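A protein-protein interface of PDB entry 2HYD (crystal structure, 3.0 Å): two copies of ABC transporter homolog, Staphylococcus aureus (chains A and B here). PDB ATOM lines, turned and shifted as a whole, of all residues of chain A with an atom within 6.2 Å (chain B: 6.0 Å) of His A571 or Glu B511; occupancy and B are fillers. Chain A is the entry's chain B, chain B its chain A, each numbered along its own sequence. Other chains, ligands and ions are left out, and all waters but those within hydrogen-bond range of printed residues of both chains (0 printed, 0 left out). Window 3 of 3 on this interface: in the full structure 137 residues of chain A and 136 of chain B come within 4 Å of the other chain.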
ATOM      1  N   MET A 375     -13.892   6.454 -10.500  1.00  0.00           N
ATOM      2  CA  MET A 375     -13.052   5.786  -9.522  1.00  0.00           C
ATOM      3  C   MET A 375     -11.707   6.505  -9.571  1.00  0.00           C
ATOM      4  O   MET A 375     -11.357   7.122 -10.578  1.00  0.00           O
ATOM      5  CB  MET A 375     -12.882   4.306  -9.878  1.00  0.00           C
ATOM      6  CG  MET A 375     -14.195   3.510  -9.909  1.00  0.00           C
ATOM      7  SD  MET A 375     -14.128   2.015 -10.982  1.00  0.00           S
ATOM      8  CE  MET A 375     -15.713   1.183 -10.613  1.00  0.00           C
ATOM      9  N   GLN A 566     -29.653   5.025 -14.570  1.00  0.00           N
ATOM     10  CA  GLN A 566     -29.333   4.006 -13.569  1.00  0.00           C
ATOM     11  C   GLN A 566     -28.065   3.249 -13.962  1.00  0.00           C
ATOM     12  O   GLN A 566     -27.956   2.020 -13.808  1.00  0.00           O
ATOM     13  CB  GLN A 566     -30.510   3.052 -13.378  1.00  0.00           C
ATOM     14  CG  GLN A 566     -31.686   3.713 -12.685  1.00  0.00           C
ATOM     15  CD  GLN A 566     -32.744   2.720 -12.264  1.00  0.00           C
ATOM     16  OE1 GLN A 566     -32.446   1.720 -11.614  1.00  0.00           O
ATOM     17  NE2 GLN A 566     -33.988   2.994 -12.623  1.00  0.00           N
ATOM     18  N   GLY A 567     -27.102   4.013 -14.463  1.00  0.00           N
ATOM     19  CA  GLY A 567     -25.852   3.439 -14.900  1.00  0.00           C
ATOM     20  C   GLY A 567     -24.677   3.715 -13.991  1.00  0.00           C
ATOM     21  O   GLY A 567     -24.817   3.822 -12.774  1.00  0.00           O
ATOM     22  N   ALA A 568     -23.507   3.830 -14.609  1.00  0.00           N
ATOM     23  CA  ALA A 568     -22.274   4.066 -13.890  1.00  0.00           C
ATOM     24  C   ALA A 568     -22.404   5.188 -12.881  1.00  0.00           C
ATOM     25  O   ALA A 568     -22.129   4.993 -11.697  1.00  0.00           O
ATOM     26  CB  ALA A 568     -21.155   4.378 -14.871  1.00  0.00           C
ATOM     27  N   TYR A 569     -22.828   6.358 -13.353  1.00  0.00           N
ATOM     28  CA  TYR A 569     -22.955   7.535 -12.495  1.00  0.00           C
ATOM     29  C   TYR A 569     -23.846   7.296 -11.286  1.00  0.00           C
ATOM     30  O   TYR A 569     -23.422   7.468 -10.141  1.00  0.00           O
ATOM     31  CB  TYR A 569     -23.487   8.732 -13.288  1.00  0.00           C
ATOM     32  CG  TYR A 569     -23.586   9.979 -12.439  1.00  0.00           C
ATOM     33  CD1 TYR A 569     -22.435  10.667 -12.033  1.00  0.00           C
ATOM     34  CD2 TYR A 569     -24.825  10.437 -11.980  1.00  0.00           C
ATOM     35  CE1 TYR A 569     -22.516  11.774 -11.191  1.00  0.00           C
ATOM     36  CE2 TYR A 569     -24.917  11.543 -11.139  1.00  0.00           C
ATOM     37  CZ  TYR A 569     -23.760  12.200 -10.751  1.00  0.00           C
ATOM     38  OH  TYR A 569     -23.867  13.286  -9.934  1.00  0.00           O
ATOM     39  N   GLU A 570     -25.087   6.911 -11.555  1.00  0.00           N
ATOM     40  CA  GLU A 570     -26.048   6.644 -10.498  1.00  0.00           C
ATOM     41  C   GLU A 570     -25.412   5.722  -9.461  1.00  0.00           C
ATOM     42  O   GLU A 570     -25.491   5.981  -8.271  1.00  0.00           O
ATOM     43  CB  GLU A 570     -27.318   6.026 -11.106  1.00  0.00           C
ATOM     44  CG  GLU A 570     -28.457   5.761 -10.134  1.00  0.00           C
ATOM     45  CD  GLU A 570     -28.352   4.399  -9.468  1.00  0.00           C
ATOM     46  OE1 GLU A 570     -27.366   4.165  -8.744  1.00  0.00           O
ATOM     47  OE2 GLU A 570     -29.253   3.555  -9.673  1.00  0.00           O
ATOM     48  N   HIS A 571     -24.761   4.659  -9.919  1.00  0.00           N
ATOM     49  CA  HIS A 571     -24.111   3.713  -9.022  1.00  0.00           C
ATOM     50  C   HIS A 571     -23.342   4.454  -7.935  1.00  0.00           C
ATOM     51  O   HIS A 571     -23.580   4.253  -6.745  1.00  0.00           O
ATOM     52  CB  HIS A 571     -23.152   2.817  -9.812  1.00  0.00           C
ATOM     53  CG  HIS A 571     -22.331   1.897  -8.956  1.00  0.00           C
ATOM     54  ND1 HIS A 571     -22.860   0.783  -8.339  1.00  0.00           N
ATOM     55  CD2 HIS A 571     -21.021   1.932  -8.611  1.00  0.00           C
ATOM     56  CE1 HIS A 571     -21.910   0.172  -7.651  1.00  0.00           C
ATOM     57  NE2 HIS A 571     -20.784   0.849  -7.799  1.00  0.00           N
ATOM     58  N   LEU A 572     -22.417   5.307  -8.363  1.00  0.00           N
ATOM     59  CA  LEU A 572     -21.588   6.106  -7.462  1.00  0.00           C
ATOM     60  C   LEU A 572     -22.411   7.038  -6.568  1.00  0.00           C
ATOM     61  O   LEU A 572     -22.308   7.007  -5.337  1.00  0.00           O
ATOM     62  CB  LEU A 572     -20.606   6.945  -8.273  1.00  0.00           C
ATOM     63  CG  LEU A 572     -19.145   6.531  -8.232  1.00  0.00           C
ATOM     64  CD1 LEU A 572     -18.350   7.505  -9.063  1.00  0.00           C
ATOM     65  CD2 LEU A 572     -18.642   6.525  -6.800  1.00  0.00           C
ATOM     66  N   TYR A 573     -23.217   7.885  -7.194  1.00  0.00           N
ATOM     67  CA  TYR A 573     -24.050   8.813  -6.444  1.00  0.00           C
ATOM     68  C   TYR A 573     -24.817   7.993  -5.421  1.00  0.00           C
ATOM     69  O   TYR A 573     -24.714   8.216  -4.222  1.00  0.00           O
ATOM     70  CB  TYR A 573     -25.027   9.511  -7.383  1.00  0.00           C
ATOM     71  CG  TYR A 573     -25.649  10.736  -6.786  1.00  0.00           C
ATOM     72  CD1 TYR A 573     -24.893  11.884  -6.574  1.00  0.00           C
ATOM     73  CD2 TYR A 573     -26.984  10.744  -6.401  1.00  0.00           C
ATOM     74  CE1 TYR A 573     -25.450  13.014  -5.988  1.00  0.00           C
ATOM     75  CE2 TYR A 573     -27.553  11.868  -5.812  1.00  0.00           C
ATOM     76  CZ  TYR A 573     -26.778  12.998  -5.607  1.00  0.00           C
ATOM     77  OH  TYR A 573     -27.326  14.107  -5.015  1.00  0.00           O
ATOM     78  N   SER A 574     -25.565   7.024  -5.930  1.00  0.00           N
ATOM     79  CA  SER A 574     -26.381   6.121  -5.134  1.00  0.00           C
ATOM     80  C   SER A 574     -25.682   5.605  -3.878  1.00  0.00           C
ATOM     81  O   SER A 574     -26.339   5.165  -2.942  1.00  0.00           O
ATOM     82  CB  SER A 574     -26.806   4.939  -6.004  1.00  0.00           C
ATOM     83  OG  SER A 574     -27.815   4.166  -5.384  1.00  0.00           O
ATOM     84  N   ILE A 575     -24.357   5.657  -3.848  1.00  0.00           N
ATOM     85  CA  ILE A 575     -23.611   5.173  -2.693  1.00  0.00           C
ATOM     86  C   ILE A 575     -23.605   6.147  -1.507  1.00  0.00           C
ATOM     87  O   ILE A 575     -23.255   5.770  -0.376  1.00  0.00           O
ATOM     88  CB  ILE A 575     -22.159   4.831  -3.098  1.00  0.00           C
ATOM     89  CG1 ILE A 575     -22.181   3.677  -4.099  1.00  0.00           C
ATOM     90  CG2 ILE A 575     -21.327   4.462  -1.884  1.00  0.00           C
ATOM     91  CD1 ILE A 575     -20.816   3.203  -4.528  1.00  0.00           C
ATOM     92  N   GLN A 576     -24.023   7.387  -1.758  1.00  0.00           N
ATOM     93  CA  GLN A 576     -24.034   8.419  -0.727  1.00  0.00           C
ATOM     94  C   GLN A 576     -25.046   8.266   0.382  1.00  0.00           C
ATOM     95  O   GLN A 576     -24.692   7.974   1.518  1.00  0.00           O
ATOM     96  CB  GLN A 576     -24.221   9.784  -1.359  1.00  0.00           C
ATOM     97  CG  GLN A 576     -23.035  10.204  -2.192  1.00  0.00           C
ATOM     98  CD  GLN A 576     -23.194  11.583  -2.788  1.00  0.00           C
ATOM     99  OE1 GLN A 576     -24.188  11.865  -3.461  1.00  0.00           O
ATOM    100  NE2 GLN A 576     -22.207  12.451  -2.556  1.00  0.00           N
ATOM    101  N   ASP B 509     -12.757   8.397  -4.182  1.00  0.00           N
ATOM    102  CA  ASP B 509     -14.107   8.502  -4.728  1.00  0.00           C
ATOM    103  C   ASP B 509     -15.061   7.893  -3.715  1.00  0.00           C
ATOM    104  O   ASP B 509     -14.621   7.329  -2.709  1.00  0.00           O
ATOM    105  CB  ASP B 509     -14.209   7.711  -6.014  1.00  0.00           C
ATOM    106  CG  ASP B 509     -13.784   6.290  -5.831  1.00  0.00           C
ATOM    107  OD1 ASP B 509     -12.555   6.057  -5.774  1.00  0.00           O
ATOM    108  OD2 ASP B 509     -14.681   5.427  -5.722  1.00  0.00           O
ATOM    109  N   LEU B 510     -16.361   7.963  -3.985  1.00  0.00           N
ATOM    110  CA  LEU B 510     -17.322   7.419  -3.036  1.00  0.00           C
ATOM    111  C   LEU B 510     -17.116   5.923  -2.814  1.00  0.00           C
ATOM    112  O   LEU B 510     -17.079   5.454  -1.675  1.00  0.00           O
ATOM    113  CB  LEU B 510     -18.748   7.706  -3.503  1.00  0.00           C
ATOM    114  CG  LEU B 510     -19.121   9.192  -3.535  1.00  0.00           C
ATOM    115  CD1 LEU B 510     -20.551   9.336  -3.996  1.00  0.00           C
ATOM    116  CD2 LEU B 510     -18.955   9.816  -2.165  1.00  0.00           C
ATOM    117  N   GLU B 511     -16.939   5.192  -3.910  1.00  0.00           N
ATOM    118  CA  GLU B 511     -16.754   3.745  -3.868  1.00  0.00           C
ATOM    119  C   GLU B 511     -15.539   3.277  -3.060  1.00  0.00           C
ATOM    120  O   GLU B 511     -15.673   2.520  -2.104  1.00  0.00           O
ATOM    121  CB  GLU B 511     -16.687   3.225  -5.308  1.00  0.00           C
ATOM    122  CG  GLU B 511     -16.650   1.712  -5.484  1.00  0.00           C
ATOM    123  CD  GLU B 511     -17.105   1.286  -6.883  1.00  0.00           C
ATOM    124  OE1 GLU B 511     -16.879   2.048  -7.860  1.00  0.00           O
ATOM    125  OE2 GLU B 511     -17.687   0.185  -7.006  1.00  0.00           O
ATOM    126  N   SER B 512     -14.356   3.738  -3.435  1.00  0.00           N
ATOM    127  CA  SER B 512     -13.140   3.341  -2.751  1.00  0.00           C
ATOM    128  C   SER B 512     -13.287   3.590  -1.272  1.00  0.00           C
ATOM    129  O   SER B 512     -12.838   2.796  -0.437  1.00  0.00           O
ATOM    130  CB  SER B 512     -11.966   4.145  -3.271  1.00  0.00           C
ATOM    131  OG  SER B 512     -12.023   4.205  -4.674  1.00  0.00           O
ATOM    132  N   GLU B 513     -13.910   4.717  -0.957  1.00  0.00           N
ATOM    133  CA  GLU B 513     -14.126   5.115   0.420  1.00  0.00           C
ATOM    134  C   GLU B 513     -14.896   4.025   1.150  1.00  0.00           C
ATOM    135  O   GLU B 513     -14.538   3.636   2.259  1.00  0.00           O
ATOM    136  CB  GLU B 513     -14.900   6.425   0.444  1.00  0.00           C
ATOM    137  CG  GLU B 513     -15.106   7.010   1.814  1.00  0.00           C
ATOM    138  CD  GLU B 513     -15.726   8.383   1.748  1.00  0.00           C
ATOM    139  OE1 GLU B 513     -16.712   8.545   1.000  1.00  0.00           O
ATOM    140  OE2 GLU B 513     -15.234   9.297   2.443  1.00  0.00           O
ATOM    141  N   SER B 514     -15.948   3.532   0.502  1.00  0.00           N
ATOM    142  CA  SER B 514     -16.799   2.474   1.058  1.00  0.00           C
ATOM    143  C   SER B 514     -15.929   1.308   1.466  1.00  0.00           C
ATOM    144  O   SER B 514     -16.042   0.797   2.581  1.00  0.00           O
ATOM    145  CB  SER B 514     -17.793   1.958   0.018  1.00  0.00           C
ATOM    146  OG  SER B 514     -18.476   3.014  -0.618  1.00  0.00           O
ATOM    147  N   ILE B 515     -15.072   0.887   0.540  1.00  0.00           N
ATOM    148  CA  ILE B 515     -14.186  -0.230   0.782  1.00  0.00           C
ATOM    149  C   ILE B 515     -13.357   0.046   2.013  1.00  0.00           C
ATOM    150  O   ILE B 515     -13.501  -0.626   3.028  1.00  0.00           O
ATOM    151  CB  ILE B 515     -13.226  -0.463  -0.395  1.00  0.00           C
ATOM    152  CG1 ILE B 515     -13.967  -0.339  -1.728  1.00  0.00           C
ATOM    153  CG2 ILE B 515     -12.609  -1.837  -0.281  1.00  0.00           C
ATOM    154  CD1 ILE B 515     -15.140  -1.236  -1.859  1.00  0.00           C
ATOM    155  N   ILE B 516     -12.488   1.041   1.924  1.00  0.00           N
ATOM    156  CA  ILE B 516     -11.638   1.369   3.051  1.00  0.00           C
ATOM    157  C   ILE B 516     -12.439   1.523   4.326  1.00  0.00           C
ATOM    158  O   ILE B 516     -11.967   1.189   5.411  1.00  0.00           O
ATOM    159  CB  ILE B 516     -10.857   2.647   2.795  1.00  0.00           C
ATOM    160  CG1 ILE B 516      -9.904   2.415   1.630  1.00  0.00           C
ATOM    161  CG2 ILE B 516     -10.098   3.051   4.052  1.00  0.00           C
ATOM    162  CD1 ILE B 516      -8.941   3.524   1.403  1.00  0.00           C
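Of the printed residues of chain B, Met A375 touches Asp B509 (3.8 Å) and Glu B511 (3.1 Å).
Gly A567 touches none of the printed residues of chain B.
Of chain B, only Glu B511 comes within 4 Å of His A571.
Of the printed residues of chain B, Ile A575 touches Ser B514.
Of chain A, only Met A375 (3.1 Å), His A571 (3.3 Å) and Leu A572 (3.6 Å) come within 4 Å of Glu B511.
Ser B512 touches none of the printed residues of chain A.
Printed residues of chain A within 4 Å of Ser B514: Ile A575.
The nearest printed residue of chain B that does not touch His A571 is Leu B510 (6.5 Å).
The nearest residue of chain A that does not touch Glu B511 is Ile A575 (4.2 Å).
The nearest printed residue of chain A that does not touch Ser B514 is Leu A572 (7.1 Å).
The side-chain carboxylate of Asp B509 is in hydrogen-bond range of the backbone NH of Glu B511, 2.9 Å away.
The side-chain carboxylate of Asp B509 lies within hydrogen-bond range of the backbone NH of Ser B512 (2.9 Å).
OG of Ser B514 sits at hydrogen-bond distance from O of Leu B510.
The backbone carbonyl oxygen (O) of Glu B511 lies close to the side-chain hydroxyl (OG) of Ser B514.
The side-chain carboxylate of Glu B511 is in hydrogen-bond range of a ring nitrogen (NE2) of His A571 (3.3 Å).
CA of Met A375 touches OD1 of Asp B509, at 3.8 Å.
OE1 of Glu B511 touches CE of Met A375 (3.1 Å).
O of Leu A572 touches CD1 of Leu B510, at 3.2 Å.
Leu A572 touches Glu B511.
CG2 of Ile A575 touches OG of Ser B514 (3.4 Å).
CG of Gln A576 touches CD1 of Leu B510 (3.2 Å).
No position is printed for both chains.
Of the 7 pairs that touch across the chains among the printed residues, none has its exchanged pair printed and touching as well.
Of the 12 printed residues of chain A, 5 touch a printed residue of chain B.
Hydrophobic or aromatic side chains of chain A within 4 Å of the printed part of chain B: Met A375, His A571, Leu A572 and Ile A575.
Of the 8 printed residues of chain B, 4 touch a printed residue of chain A.
Hydrophobic or aromatic side chains of chain B within 4 Å of the printed part of chain A: Leu B510.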
